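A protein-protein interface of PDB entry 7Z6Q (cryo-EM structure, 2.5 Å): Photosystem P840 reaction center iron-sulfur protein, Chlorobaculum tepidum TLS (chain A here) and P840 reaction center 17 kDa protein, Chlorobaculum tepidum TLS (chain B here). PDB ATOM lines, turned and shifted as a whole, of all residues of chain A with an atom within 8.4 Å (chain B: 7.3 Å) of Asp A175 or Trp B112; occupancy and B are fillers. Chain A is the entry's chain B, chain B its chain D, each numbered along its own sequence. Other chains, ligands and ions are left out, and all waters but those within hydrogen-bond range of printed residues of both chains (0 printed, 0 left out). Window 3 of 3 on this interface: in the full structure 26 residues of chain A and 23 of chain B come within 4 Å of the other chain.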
ATOM      1  N   TYR A 133      21.480 -21.389  24.977  1.00  0.00           N
ATOM      2  CA  TYR A 133      20.982 -22.720  25.289  1.00  0.00           C
ATOM      3  C   TYR A 133      20.987 -23.572  24.033  1.00  0.00           C
ATOM      4  O   TYR A 133      20.715 -23.076  22.936  1.00  0.00           O
ATOM      5  CB  TYR A 133      19.573 -22.641  25.887  1.00  0.00           C
ATOM      6  CG  TYR A 133      19.566 -21.946  27.226  1.00  0.00           C
ATOM      7  CD1 TYR A 133      19.879 -22.634  28.386  1.00  0.00           C
ATOM      8  CD2 TYR A 133      19.273 -20.594  27.325  1.00  0.00           C
ATOM      9  CE1 TYR A 133      19.883 -21.999  29.602  1.00  0.00           C
ATOM     10  CE2 TYR A 133      19.286 -19.951  28.538  1.00  0.00           C
ATOM     11  CZ  TYR A 133      19.593 -20.659  29.672  1.00  0.00           C
ATOM     12  OH  TYR A 133      19.604 -20.019  30.888  1.00  0.00           O
ATOM     13  N   PHE A 134      21.291 -24.856  24.199  1.00  0.00           N
ATOM     14  CA  PHE A 134      21.519 -25.709  23.045  1.00  0.00           C
ATOM     15  C   PHE A 134      21.045 -27.126  23.336  1.00  0.00           C
ATOM     16  O   PHE A 134      20.969 -27.542  24.494  1.00  0.00           O
ATOM     17  CB  PHE A 134      23.004 -25.731  22.672  1.00  0.00           C
ATOM     18  CG  PHE A 134      23.597 -24.376  22.395  1.00  0.00           C
ATOM     19  CD1 PHE A 134      23.442 -23.778  21.157  1.00  0.00           C
ATOM     20  CD2 PHE A 134      24.319 -23.707  23.369  1.00  0.00           C
ATOM     21  CE1 PHE A 134      23.991 -22.538  20.897  1.00  0.00           C
ATOM     22  CE2 PHE A 134      24.867 -22.463  23.114  1.00  0.00           C
ATOM     23  CZ  PHE A 134      24.700 -21.880  21.875  1.00  0.00           C
ATOM     24  N   ILE A 135      20.742 -27.866  22.270  1.00  0.00           N
ATOM     25  CA  ILE A 135      20.461 -29.296  22.350  1.00  0.00           C
ATOM     26  C   ILE A 135      21.689 -30.047  21.873  1.00  0.00           C
ATOM     27  O   ILE A 135      22.212 -29.771  20.787  1.00  0.00           O
ATOM     28  CB  ILE A 135      19.246 -29.703  21.499  1.00  0.00           C
ATOM     29  CG1 ILE A 135      18.126 -28.679  21.577  1.00  0.00           C
ATOM     30  CG2 ILE A 135      18.739 -31.070  21.929  1.00  0.00           C
ATOM     31  CD1 ILE A 135      17.575 -28.493  22.936  1.00  0.00           C
ATOM     32  N   ILE A 136      22.139 -31.010  22.669  1.00  0.00           N
ATOM     33  CA  ILE A 136      23.146 -31.946  22.192  1.00  0.00           C
ATOM     34  C   ILE A 136      22.401 -33.054  21.452  1.00  0.00           C
ATOM     35  O   ILE A 136      21.768 -33.910  22.070  1.00  0.00           O
ATOM     36  CB  ILE A 136      24.000 -32.503  23.323  1.00  0.00           C
ATOM     37  CG1 ILE A 136      24.573 -31.392  24.193  1.00  0.00           C
ATOM     38  CG2 ILE A 136      25.121 -33.169  22.717  1.00  0.00           C
ATOM     39  CD1 ILE A 136      25.410 -31.916  25.335  1.00  0.00           C
ATOM     40  N   GLU A 137      22.498 -33.057  20.124  1.00  0.00           N
ATOM     41  CA  GLU A 137      21.545 -33.805  19.311  1.00  0.00           C
ATOM     42  C   GLU A 137      21.676 -35.314  19.480  1.00  0.00           C
ATOM     43  O   GLU A 137      20.669 -36.027  19.432  1.00  0.00           O
ATOM     44  CB  GLU A 137      21.705 -33.408  17.850  1.00  0.00           C
ATOM     45  CG  GLU A 137      21.342 -31.958  17.595  1.00  0.00           C
ATOM     46  CD  GLU A 137      19.926 -31.609  17.999  1.00  0.00           C
ATOM     47  OE1 GLU A 137      19.070 -32.517  18.022  1.00  0.00           O
ATOM     48  OE2 GLU A 137      19.666 -30.420  18.278  1.00  0.00           O
ATOM     49  N   CYS A 150       9.135 -23.258  26.166  1.00  0.00           N
ATOM     50  CA  CYS A 150       9.424 -22.095  25.340  1.00  0.00           C
ATOM     51  C   CYS A 150       8.143 -21.311  25.083  1.00  0.00           C
ATOM     52  O   CYS A 150       7.119 -21.909  24.738  1.00  0.00           O
ATOM     53  CB  CYS A 150      10.055 -22.528  24.019  1.00  0.00           C
ATOM     54  SG  CYS A 150      11.006 -21.244  23.187  1.00  0.00           S
ATOM     55  N   VAL A 154       7.472 -17.153  20.892  1.00  0.00           N
ATOM     56  CA  VAL A 154       8.889 -17.281  20.557  1.00  0.00           C
ATOM     57  C   VAL A 154       9.108 -18.764  20.272  1.00  0.00           C
ATOM     58  O   VAL A 154       9.440 -19.544  21.168  1.00  0.00           O
ATOM     59  CB  VAL A 154       9.808 -16.787  21.678  1.00  0.00           C
ATOM     60  CG1 VAL A 154      11.251 -16.740  21.208  1.00  0.00           C
ATOM     61  CG2 VAL A 154       9.354 -15.421  22.175  1.00  0.00           C
ATOM     62  N   ASN A 155       8.934 -19.162  19.015  1.00  0.00           N
ATOM     63  CA  ASN A 155       8.960 -20.578  18.650  1.00  0.00           C
ATOM     64  C   ASN A 155      10.393 -21.028  18.362  1.00  0.00           C
ATOM     65  O   ASN A 155      10.749 -21.429  17.255  1.00  0.00           O
ATOM     66  CB  ASN A 155       8.042 -20.826  17.459  1.00  0.00           C
ATOM     67  CG  ASN A 155       7.368 -22.181  17.515  1.00  0.00           C
ATOM     68  OD1 ASN A 155       7.307 -22.815  18.567  1.00  0.00           O
ATOM     69  ND2 ASN A 155       6.855 -22.632  16.377  1.00  0.00           N
ATOM     70  N   ALA A 156      11.221 -20.961  19.404  1.00  0.00           N
ATOM     71  CA  ALA A 156      12.639 -21.265  19.250  1.00  0.00           C
ATOM     72  C   ALA A 156      12.878 -22.762  19.108  1.00  0.00           C
ATOM     73  O   ALA A 156      13.467 -23.210  18.120  1.00  0.00           O
ATOM     74  CB  ALA A 156      13.426 -20.709  20.436  1.00  0.00           C
ATOM     75  N   ILE A 157      12.489 -23.532  20.123  1.00  0.00           N
ATOM     76  CA  ILE A 157      12.673 -25.010  20.051  1.00  0.00           C
ATOM     77  C   ILE A 157      11.731 -25.561  18.976  1.00  0.00           C
ATOM     78  O   ILE A 157      10.616 -25.027  18.814  1.00  0.00           O
ATOM     79  CB  ILE A 157      12.467 -25.691  21.418  1.00  0.00           C
ATOM     80  CG1 ILE A 157      13.545 -25.283  22.425  1.00  0.00           C
ATOM     81  CG2 ILE A 157      12.387 -27.200  21.267  1.00  0.00           C
ATOM     82  CD1 ILE A 157      13.254 -25.705  23.842  1.00  0.00           C
ATOM     83  N   GLY A 158      12.191 -26.584  18.259  1.00  0.00           N
ATOM     84  CA  GLY A 158      11.434 -27.221  17.202  1.00  0.00           C
ATOM     85  C   GLY A 158      11.902 -28.644  16.995  1.00  0.00           C
ATOM     86  O   GLY A 158      12.885 -29.095  17.589  1.00  0.00           O
ATOM     87  N   LYS A 160      12.792 -32.076  14.417  1.00  0.00           N
ATOM     88  CA  LYS A 160      13.536 -32.420  13.207  1.00  0.00           C
ATOM     89  C   LYS A 160      13.484 -33.925  12.986  1.00  0.00           C
ATOM     90  O   LYS A 160      14.069 -34.682  13.766  1.00  0.00           O
ATOM     91  CB  LYS A 160      14.990 -31.957  13.319  1.00  0.00           C
ATOM     92  CG  LYS A 160      15.832 -32.090  12.059  1.00  0.00           C
ATOM     93  CD  LYS A 160      16.575 -33.412  11.959  1.00  0.00           C
ATOM     94  CE  LYS A 160      17.450 -33.429  10.711  1.00  0.00           C
ATOM     95  NZ  LYS A 160      17.634 -34.780  10.118  1.00  0.00           N
ATOM     96  N   CYS A 172      15.048 -32.493  18.977  1.00  0.00           N
ATOM     97  CA  CYS A 172      14.687 -31.112  19.236  1.00  0.00           C
ATOM     98  C   CYS A 172      15.899 -30.216  19.030  1.00  0.00           C
ATOM     99  O   CYS A 172      17.047 -30.644  19.166  1.00  0.00           O
ATOM    100  CB  CYS A 172      14.130 -30.948  20.654  1.00  0.00           C
ATOM    101  SG  CYS A 172      12.379 -31.365  20.803  1.00  0.00           S
ATOM    102  N   TYR A 173      15.637 -28.962  18.687  1.00  0.00           N
ATOM    103  CA  TYR A 173      16.746 -28.021  18.426  1.00  0.00           C
ATOM    104  C   TYR A 173      16.245 -26.598  18.665  1.00  0.00           C
ATOM    105  O   TYR A 173      15.087 -26.305  18.368  1.00  0.00           O
ATOM    106  CB  TYR A 173      17.187 -28.171  16.970  1.00  0.00           C
ATOM    107  CG  TYR A 173      16.161 -27.648  16.000  1.00  0.00           C
ATOM    108  CD1 TYR A 173      16.120 -26.308  15.667  1.00  0.00           C
ATOM    109  CD2 TYR A 173      15.192 -28.479  15.468  1.00  0.00           C
ATOM    110  CE1 TYR A 173      15.159 -25.809  14.810  1.00  0.00           C
ATOM    111  CE2 TYR A 173      14.226 -27.999  14.606  1.00  0.00           C
ATOM    112  CZ  TYR A 173      14.209 -26.659  14.276  1.00  0.00           C
ATOM    113  OH  TYR A 173      13.262 -26.172  13.424  1.00  0.00           O
ATOM    114  N   ILE A 174      17.108 -25.752  19.217  1.00  0.00           N
ATOM    115  CA  ILE A 174      16.804 -24.342  19.433  1.00  0.00           C
ATOM    116  C   ILE A 174      17.237 -23.517  18.232  1.00  0.00           C
ATOM    117  O   ILE A 174      18.408 -23.548  17.837  1.00  0.00           O
ATOM    118  CB  ILE A 174      17.497 -23.778  20.688  1.00  0.00           C
ATOM    119  CG1 ILE A 174      16.975 -24.414  21.974  1.00  0.00           C
ATOM    120  CG2 ILE A 174      17.320 -22.278  20.760  1.00  0.00           C
ATOM    121  CD1 ILE A 174      17.776 -24.099  23.168  1.00  0.00           C
ATOM    122  N   ASP A 175      16.294 -22.782  17.653  1.00  0.00           N
ATOM    123  CA  ASP A 175      16.600 -21.773  16.645  1.00  0.00           C
ATOM    124  C   ASP A 175      17.129 -20.529  17.346  1.00  0.00           C
ATOM    125  O   ASP A 175      16.377 -19.828  18.028  1.00  0.00           O
ATOM    126  CB  ASP A 175      15.349 -21.470  15.821  1.00  0.00           C
ATOM    127  CG  ASP A 175      15.565 -20.389  14.765  1.00  0.00           C
ATOM    128  OD1 ASP A 175      16.577 -19.661  14.803  1.00  0.00           O
ATOM    129  OD2 ASP A 175      14.709 -20.279  13.863  1.00  0.00           O
ATOM    130  N   GLN A 176      18.421 -20.243  17.176  1.00  0.00           N
ATOM    131  CA  GLN A 176      19.022 -19.096  17.845  1.00  0.00           C
ATOM    132  C   GLN A 176      18.583 -17.765  17.253  1.00  0.00           C
ATOM    133  O   GLN A 176      18.679 -16.742  17.936  1.00  0.00           O
ATOM    134  CB  GLN A 176      20.547 -19.194  17.802  1.00  0.00           C
ATOM    135  CG  GLN A 176      21.116 -20.351  18.597  1.00  0.00           C
ATOM    136  CD  GLN A 176      20.765 -20.283  20.066  1.00  0.00           C
ATOM    137  OE1 GLN A 176      20.773 -19.213  20.671  1.00  0.00           O
ATOM    138  NE2 GLN A 176      20.450 -21.431  20.651  1.00  0.00           N
ATOM    139  N   ALA A 177      18.105 -17.751  16.007  1.00  0.00           N
ATOM    140  CA  ALA A 177      17.674 -16.494  15.404  1.00  0.00           C
ATOM    141  C   ALA A 177      16.433 -15.937  16.087  1.00  0.00           C
ATOM    142  O   ALA A 177      16.246 -14.716  16.128  1.00  0.00           O
ATOM    143  CB  ALA A 177      17.418 -16.686  13.910  1.00  0.00           C
ATOM    144  N   ALA A 178      15.577 -16.807  16.622  1.00  0.00           N
ATOM    145  CA  ALA A 178      14.377 -16.378  17.322  1.00  0.00           C
ATOM    146  C   ALA A 178      14.456 -16.553  18.828  1.00  0.00           C
ATOM    147  O   ALA A 178      13.644 -15.961  19.543  1.00  0.00           O
ATOM    148  CB  ALA A 178      13.151 -17.140  16.799  1.00  0.00           C
ATOM    149  N   CYS A 179      15.398 -17.361  19.323  1.00  0.00           N
ATOM    150  CA  CYS A 179      15.524 -17.581  20.792  1.00  0.00           C
ATOM    151  C   CYS A 179      15.790 -16.252  21.509  1.00  0.00           C
ATOM    152  O   CYS A 179      16.583 -15.462  20.984  1.00  0.00           O
ATOM    153  CB  CYS A 179      16.637 -18.569  21.106  1.00  0.00           C
ATOM    154  SG  CYS A 179      16.831 -18.846  22.881  1.00  0.00           S
ATOM    155  N   ILE A 180      15.167 -16.025  22.673  1.00  0.00           N
ATOM    156  CA  ILE A 180      15.320 -14.727  23.402  1.00  0.00           C
ATOM    157  C   ILE A 180      16.069 -14.919  24.727  1.00  0.00           C
ATOM    158  O   ILE A 180      16.092 -13.975  25.530  1.00  0.00           O
ATOM    159  CB  ILE A 180      13.963 -14.021  23.610  1.00  0.00           C
ATOM    160  CG1 ILE A 180      13.000 -14.865  24.445  1.00  0.00           C
ATOM    161  CG2 ILE A 180      13.352 -13.592  22.286  1.00  0.00           C
ATOM    162  CD1 ILE A 180      11.752 -14.127  24.848  1.00  0.00           C
ATOM    163  N   SER A 181      16.638 -16.102  24.948  1.00  0.00           N
ATOM    164  CA  SER A 181      17.453 -16.383  26.159  1.00  0.00           C
ATOM    165  C   SER A 181      16.696 -16.128  27.475  1.00  0.00           C
ATOM    166  O   SER A 181      17.304 -15.550  28.387  1.00  0.00           O
ATOM    167  CB  SER A 181      18.772 -15.656  26.114  1.00  0.00           C
ATOM    168  OG  SER A 181      19.567 -16.143  25.046  1.00  0.00           O
ATOM    169  N   THR B  82      29.221 -25.691  18.101  1.00  0.00           N
ATOM    170  CA  THR B  82      28.842 -24.255  18.012  1.00  0.00           C
ATOM    171  C   THR B  82      29.927 -23.386  18.656  1.00  0.00           C
ATOM    172  O   THR B  82      29.687 -22.173  18.812  1.00  0.00           O
ATOM    173  CB  THR B  82      27.470 -23.984  18.639  1.00  0.00           C
ATOM    174  OG1 THR B  82      27.414 -24.662  19.894  1.00  0.00           O
ATOM    175  CG2 THR B  82      26.322 -24.420  17.757  1.00  0.00           C
ATOM    176  N   ASN B  91      29.842 -26.442  10.399  1.00  0.00           N
ATOM    177  CA  ASN B  91      28.412 -26.327  10.001  1.00  0.00           C
ATOM    178  C   ASN B  91      28.158 -26.916   8.610  1.00  0.00           C
ATOM    179  O   ASN B  91      27.171 -27.654   8.466  1.00  0.00           O
ATOM    180  CB  ASN B  91      27.916 -24.880  10.053  1.00  0.00           C
ATOM    181  CG  ASN B  91      26.410 -24.777   9.937  1.00  0.00           C
ATOM    182  OD1 ASN B  91      25.689 -25.673  10.370  1.00  0.00           O
ATOM    183  ND2 ASN B  91      25.927 -23.691   9.352  1.00  0.00           N
ATOM    184  N   ILE B  94      28.367 -30.684   8.772  1.00  0.00           N
ATOM    185  CA  ILE B  94      27.217 -31.193   9.575  1.00  0.00           C
ATOM    186  C   ILE B  94      25.956 -31.107   8.712  1.00  0.00           C
ATOM    187  O   ILE B  94      25.186 -32.084   8.690  1.00  0.00           O
ATOM    188  CB  ILE B  94      27.069 -30.391  10.887  1.00  0.00           C
ATOM    189  CG1 ILE B  94      28.258 -30.605  11.828  1.00  0.00           C
ATOM    190  CG2 ILE B  94      25.748 -30.703  11.572  1.00  0.00           C
ATOM    191  CD1 ILE B  94      28.293 -29.653  12.999  1.00  0.00           C
ATOM    192  N   ILE B  95      25.793 -29.995   7.993  1.00  0.00           N
ATOM    193  CA  ILE B  95      24.589 -29.788   7.136  1.00  0.00           C
ATOM    194  C   ILE B  95      24.572 -30.853   6.036  1.00  0.00           C
ATOM    195  O   ILE B  95      23.490 -31.406   5.775  1.00  0.00           O
ATOM    196  CB  ILE B  95      24.573 -28.362   6.554  1.00  0.00           C
ATOM    197  CG1 ILE B  95      24.298 -27.317   7.640  1.00  0.00           C
ATOM    198  CG2 ILE B  95      23.579 -28.260   5.409  1.00  0.00           C
ATOM    199  CD1 ILE B  95      24.528 -25.891   7.189  1.00  0.00           C
ATOM    200  N   GLY B 109      15.674 -26.703  10.622  1.00  0.00           N
ATOM    201  CA  GLY B 109      16.141 -27.494  11.777  1.00  0.00           C
ATOM    202  C   GLY B 109      17.453 -28.195  11.479  1.00  0.00           C
ATOM    203  O   GLY B 109      18.127 -28.627  12.433  1.00  0.00           O
ATOM    204  N   VAL B 110      17.773 -28.340  10.190  1.00  0.00           N
ATOM    205  CA  VAL B 110      19.040 -28.978   9.726  1.00  0.00           C
ATOM    206  C   VAL B 110      20.226 -28.120  10.178  1.00  0.00           C
ATOM    207  O   VAL B 110      21.256 -28.696  10.563  1.00  0.00           O
ATOM    208  CB  VAL B 110      19.041 -29.161   8.197  1.00  0.00           C
ATOM    209  CG1 VAL B 110      17.952 -30.116   7.737  1.00  0.00           C
ATOM    210  CG2 VAL B 110      18.930 -27.829   7.471  1.00  0.00           C
ATOM    211  N   LYS B 111      20.067 -26.795  10.113  1.00  0.00           N
ATOM    212  CA  LYS B 111      21.123 -25.805  10.456  1.00  0.00           C
ATOM    213  C   LYS B 111      21.544 -25.880  11.929  1.00  0.00           C
ATOM    214  O   LYS B 111      22.754 -25.764  12.200  1.00  0.00           O
ATOM    215  CB  LYS B 111      20.620 -24.384  10.184  1.00  0.00           C
ATOM    216  CG  LYS B 111      20.403 -24.028   8.722  1.00  0.00           C
ATOM    217  CD  LYS B 111      20.117 -22.556   8.508  1.00  0.00           C
ATOM    218  CE  LYS B 111      18.779 -22.131   9.073  1.00  0.00           C
ATOM    219  NZ  LYS B 111      18.464 -20.719   8.752  1.00  0.00           N
ATOM    220  N   TRP B 112      20.516 -25.790  12.779  1.00  0.00           N
ATOM    221  CA  TRP B 112      20.581 -25.665  14.257  1.00  0.00           C
ATOM    222  C   TRP B 112      20.960 -26.975  14.934  1.00  0.00           C
ATOM    223  O   TRP B 112      20.869 -27.031  16.166  1.00  0.00           O
ATOM    224  CB  TRP B 112      19.252 -25.124  14.783  1.00  0.00           C
ATOM    225  CG  TRP B 112      18.863 -23.826  14.150  1.00  0.00           C
ATOM    226  CD1 TRP B 112      17.735 -23.569  13.431  1.00  0.00           C
ATOM    227  CD2 TRP B 112      19.613 -22.601  14.174  1.00  0.00           C
ATOM    228  NE1 TRP B 112      17.729 -22.269  13.008  1.00  0.00           N
ATOM    229  CE2 TRP B 112      18.868 -21.650  13.449  1.00  0.00           C
ATOM    230  CE3 TRP B 112      20.833 -22.215  14.736  1.00  0.00           C
ATOM    231  CZ2 TRP B 112      19.307 -20.339  13.274  1.00  0.00           C
ATOM    232  CZ3 TRP B 112      21.267 -20.922  14.558  1.00  0.00           C
ATOM    233  CH2 TRP B 112      20.511 -19.996  13.840  1.00  0.00           C
ATOM    234  N   THR B 113      21.347 -27.989  14.168  1.00  0.00           N
ATOM    235  CA  THR B 113      21.789 -29.234  14.841  1.00  0.00           C
ATOM    236  C   THR B 113      23.131 -28.948  15.523  1.00  0.00           C
ATOM    237  O   THR B 113      23.936 -28.182  14.962  1.00  0.00           O
ATOM    238  CB  THR B 113      21.802 -30.423  13.879  1.00  0.00           C
ATOM    239  OG1 THR B 113      22.694 -30.076  12.822  1.00  0.00           O
ATOM    240  CG2 THR B 113      20.434 -30.730  13.315  1.00  0.00           C
ATOM    241  N   MET B 114      23.342 -29.532  16.701  1.00  0.00           N
ATOM    242  CA  MET B 114      24.585 -29.345  17.484  1.00  0.00           C
ATOM    243  C   MET B 114      25.074 -30.741  17.872  1.00  0.00           C
ATOM    244  O   MET B 114      24.232 -31.616  18.055  1.00  0.00           O
ATOM    245  CB  MET B 114      24.273 -28.523  18.735  1.00  0.00           C
ATOM    246  CG  MET B 114      25.441 -27.740  19.282  1.00  0.00           C
ATOM    247  SD  MET B 114      25.316 -27.663  21.075  1.00  0.00           S
ATOM    248  CE  MET B 114      26.040 -29.243  21.507  1.00  0.00           C
ATOM    249  N   ARG B 115      26.373 -30.990  17.903  1.00  0.00           N
ATOM    250  CA  ARG B 115      26.802 -32.348  18.313  1.00  0.00           C
ATOM    251  C   ARG B 115      27.940 -32.224  19.331  1.00  0.00           C
ATOM    252  O   ARG B 115      28.475 -31.133  19.487  1.00  0.00           O
ATOM    253  CB  ARG B 115      27.253 -33.209  17.125  1.00  0.00           C
ATOM    254  CG  ARG B 115      26.692 -32.838  15.758  1.00  0.00           C
ATOM    255  CD  ARG B 115      25.289 -33.381  15.567  1.00  0.00           C
ATOM    256  NE  ARG B 115      24.847 -33.467  14.183  1.00  0.00           N
ATOM    257  CZ  ARG B 115      24.132 -34.477  13.703  1.00  0.00           C
ATOM    258  NH1 ARG B 115      23.796 -35.480  14.499  1.00  0.00           N
ATOM    259  NH2 ARG B 115      23.763 -34.491  12.436  1.00  0.00           N
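The backbone carbonyl oxygen (O) of Tyr A173 lies within hydrogen-bond range of the backbone NH (N) of Gly A158, at 2.9 Å. The backbone carbonyl oxygen of Tyr A133 sits at hydrogen-bond distance from the side-chain amide nitrogen of Gln A176, 2.8 Å away. N of Ala A177 is in hydrogen-bond range of OD1 of Asp A175, at 2.7 Å. The backbone carbonyl oxygen (O) of Val B110 is in hydrogen-bond range of the side-chain hydroxyl (OG1) of Thr B113 (3.0 Å). The backbone NH (N) of Asp A175 sits at hydrogen-bond distance from the backbone carbonyl oxygen (O) of Ala A156.
Of the 22 printed residues of chain A, 9 touch a printed residue of chain B. Printed residues of chain B that touch a printed residue of chain A: Gly B109, Trp B112, Thr B113 and Met B114. Hydrophobic or aromatic side chains of chain B that line the printed part of chain A: Trp B112 and Met B114. Among the printed residues, 11 pairs touch across the chains.
The backbone NH of Glu A137 sits close to the backbone carbonyl oxygen of Met B114 (3.1 Å). OD1 of Asp A175 sits close to NE1 of Trp B112. The backbone carbonyl oxygen (O) of Ile A135 lies close to the side-chain sulfur (SD) of Met B114.
Asp A175 touches just one residue of chain B: Trp B112 (3.2 Å). Trp B112 touches just these residues of chain A: Tyr A173, Ile A174, Asp A175, Gln A176 and Ala A177. Thr B113 touches just one residue of chain A: Glu A137 (3.9 Å). Printed residues of chain B within 4 Å of Ala A177: Trp B112. Of the printed residues of chain B, Glu A137 touches Thr B113 (3.9 Å) and Met B114 (2.9 Å). Of the printed residues of chain B, Gln A176 touches Trp B112 (3.7 Å). Of the printed residues of chain B, Ile A135 touches Met B114. Cys A179 touches none of the printed residues of chain B. Cys A172 touches none of the printed residues of chain B. The nearest residue of chain B that does not touch Asp A175 is Lys B111 (6.4 Å).
Among the printed residues, pairs that only touch across the chains: Tyr A173 with Gly B109 (3.3 Å), Phe A134 with Met B114 (3.4 Å), Tyr A173 with Trp B112 (3.5 Å), Ile A174 with Trp B112 (3.5 Å), Ile A136 with Met B114 (3.7 Å), Gln A176 with Trp B112 (3.7 Å), Glu A137 with Thr B113 (3.9 Å) and Ala A177 with Trp B112 (3.9 Å).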
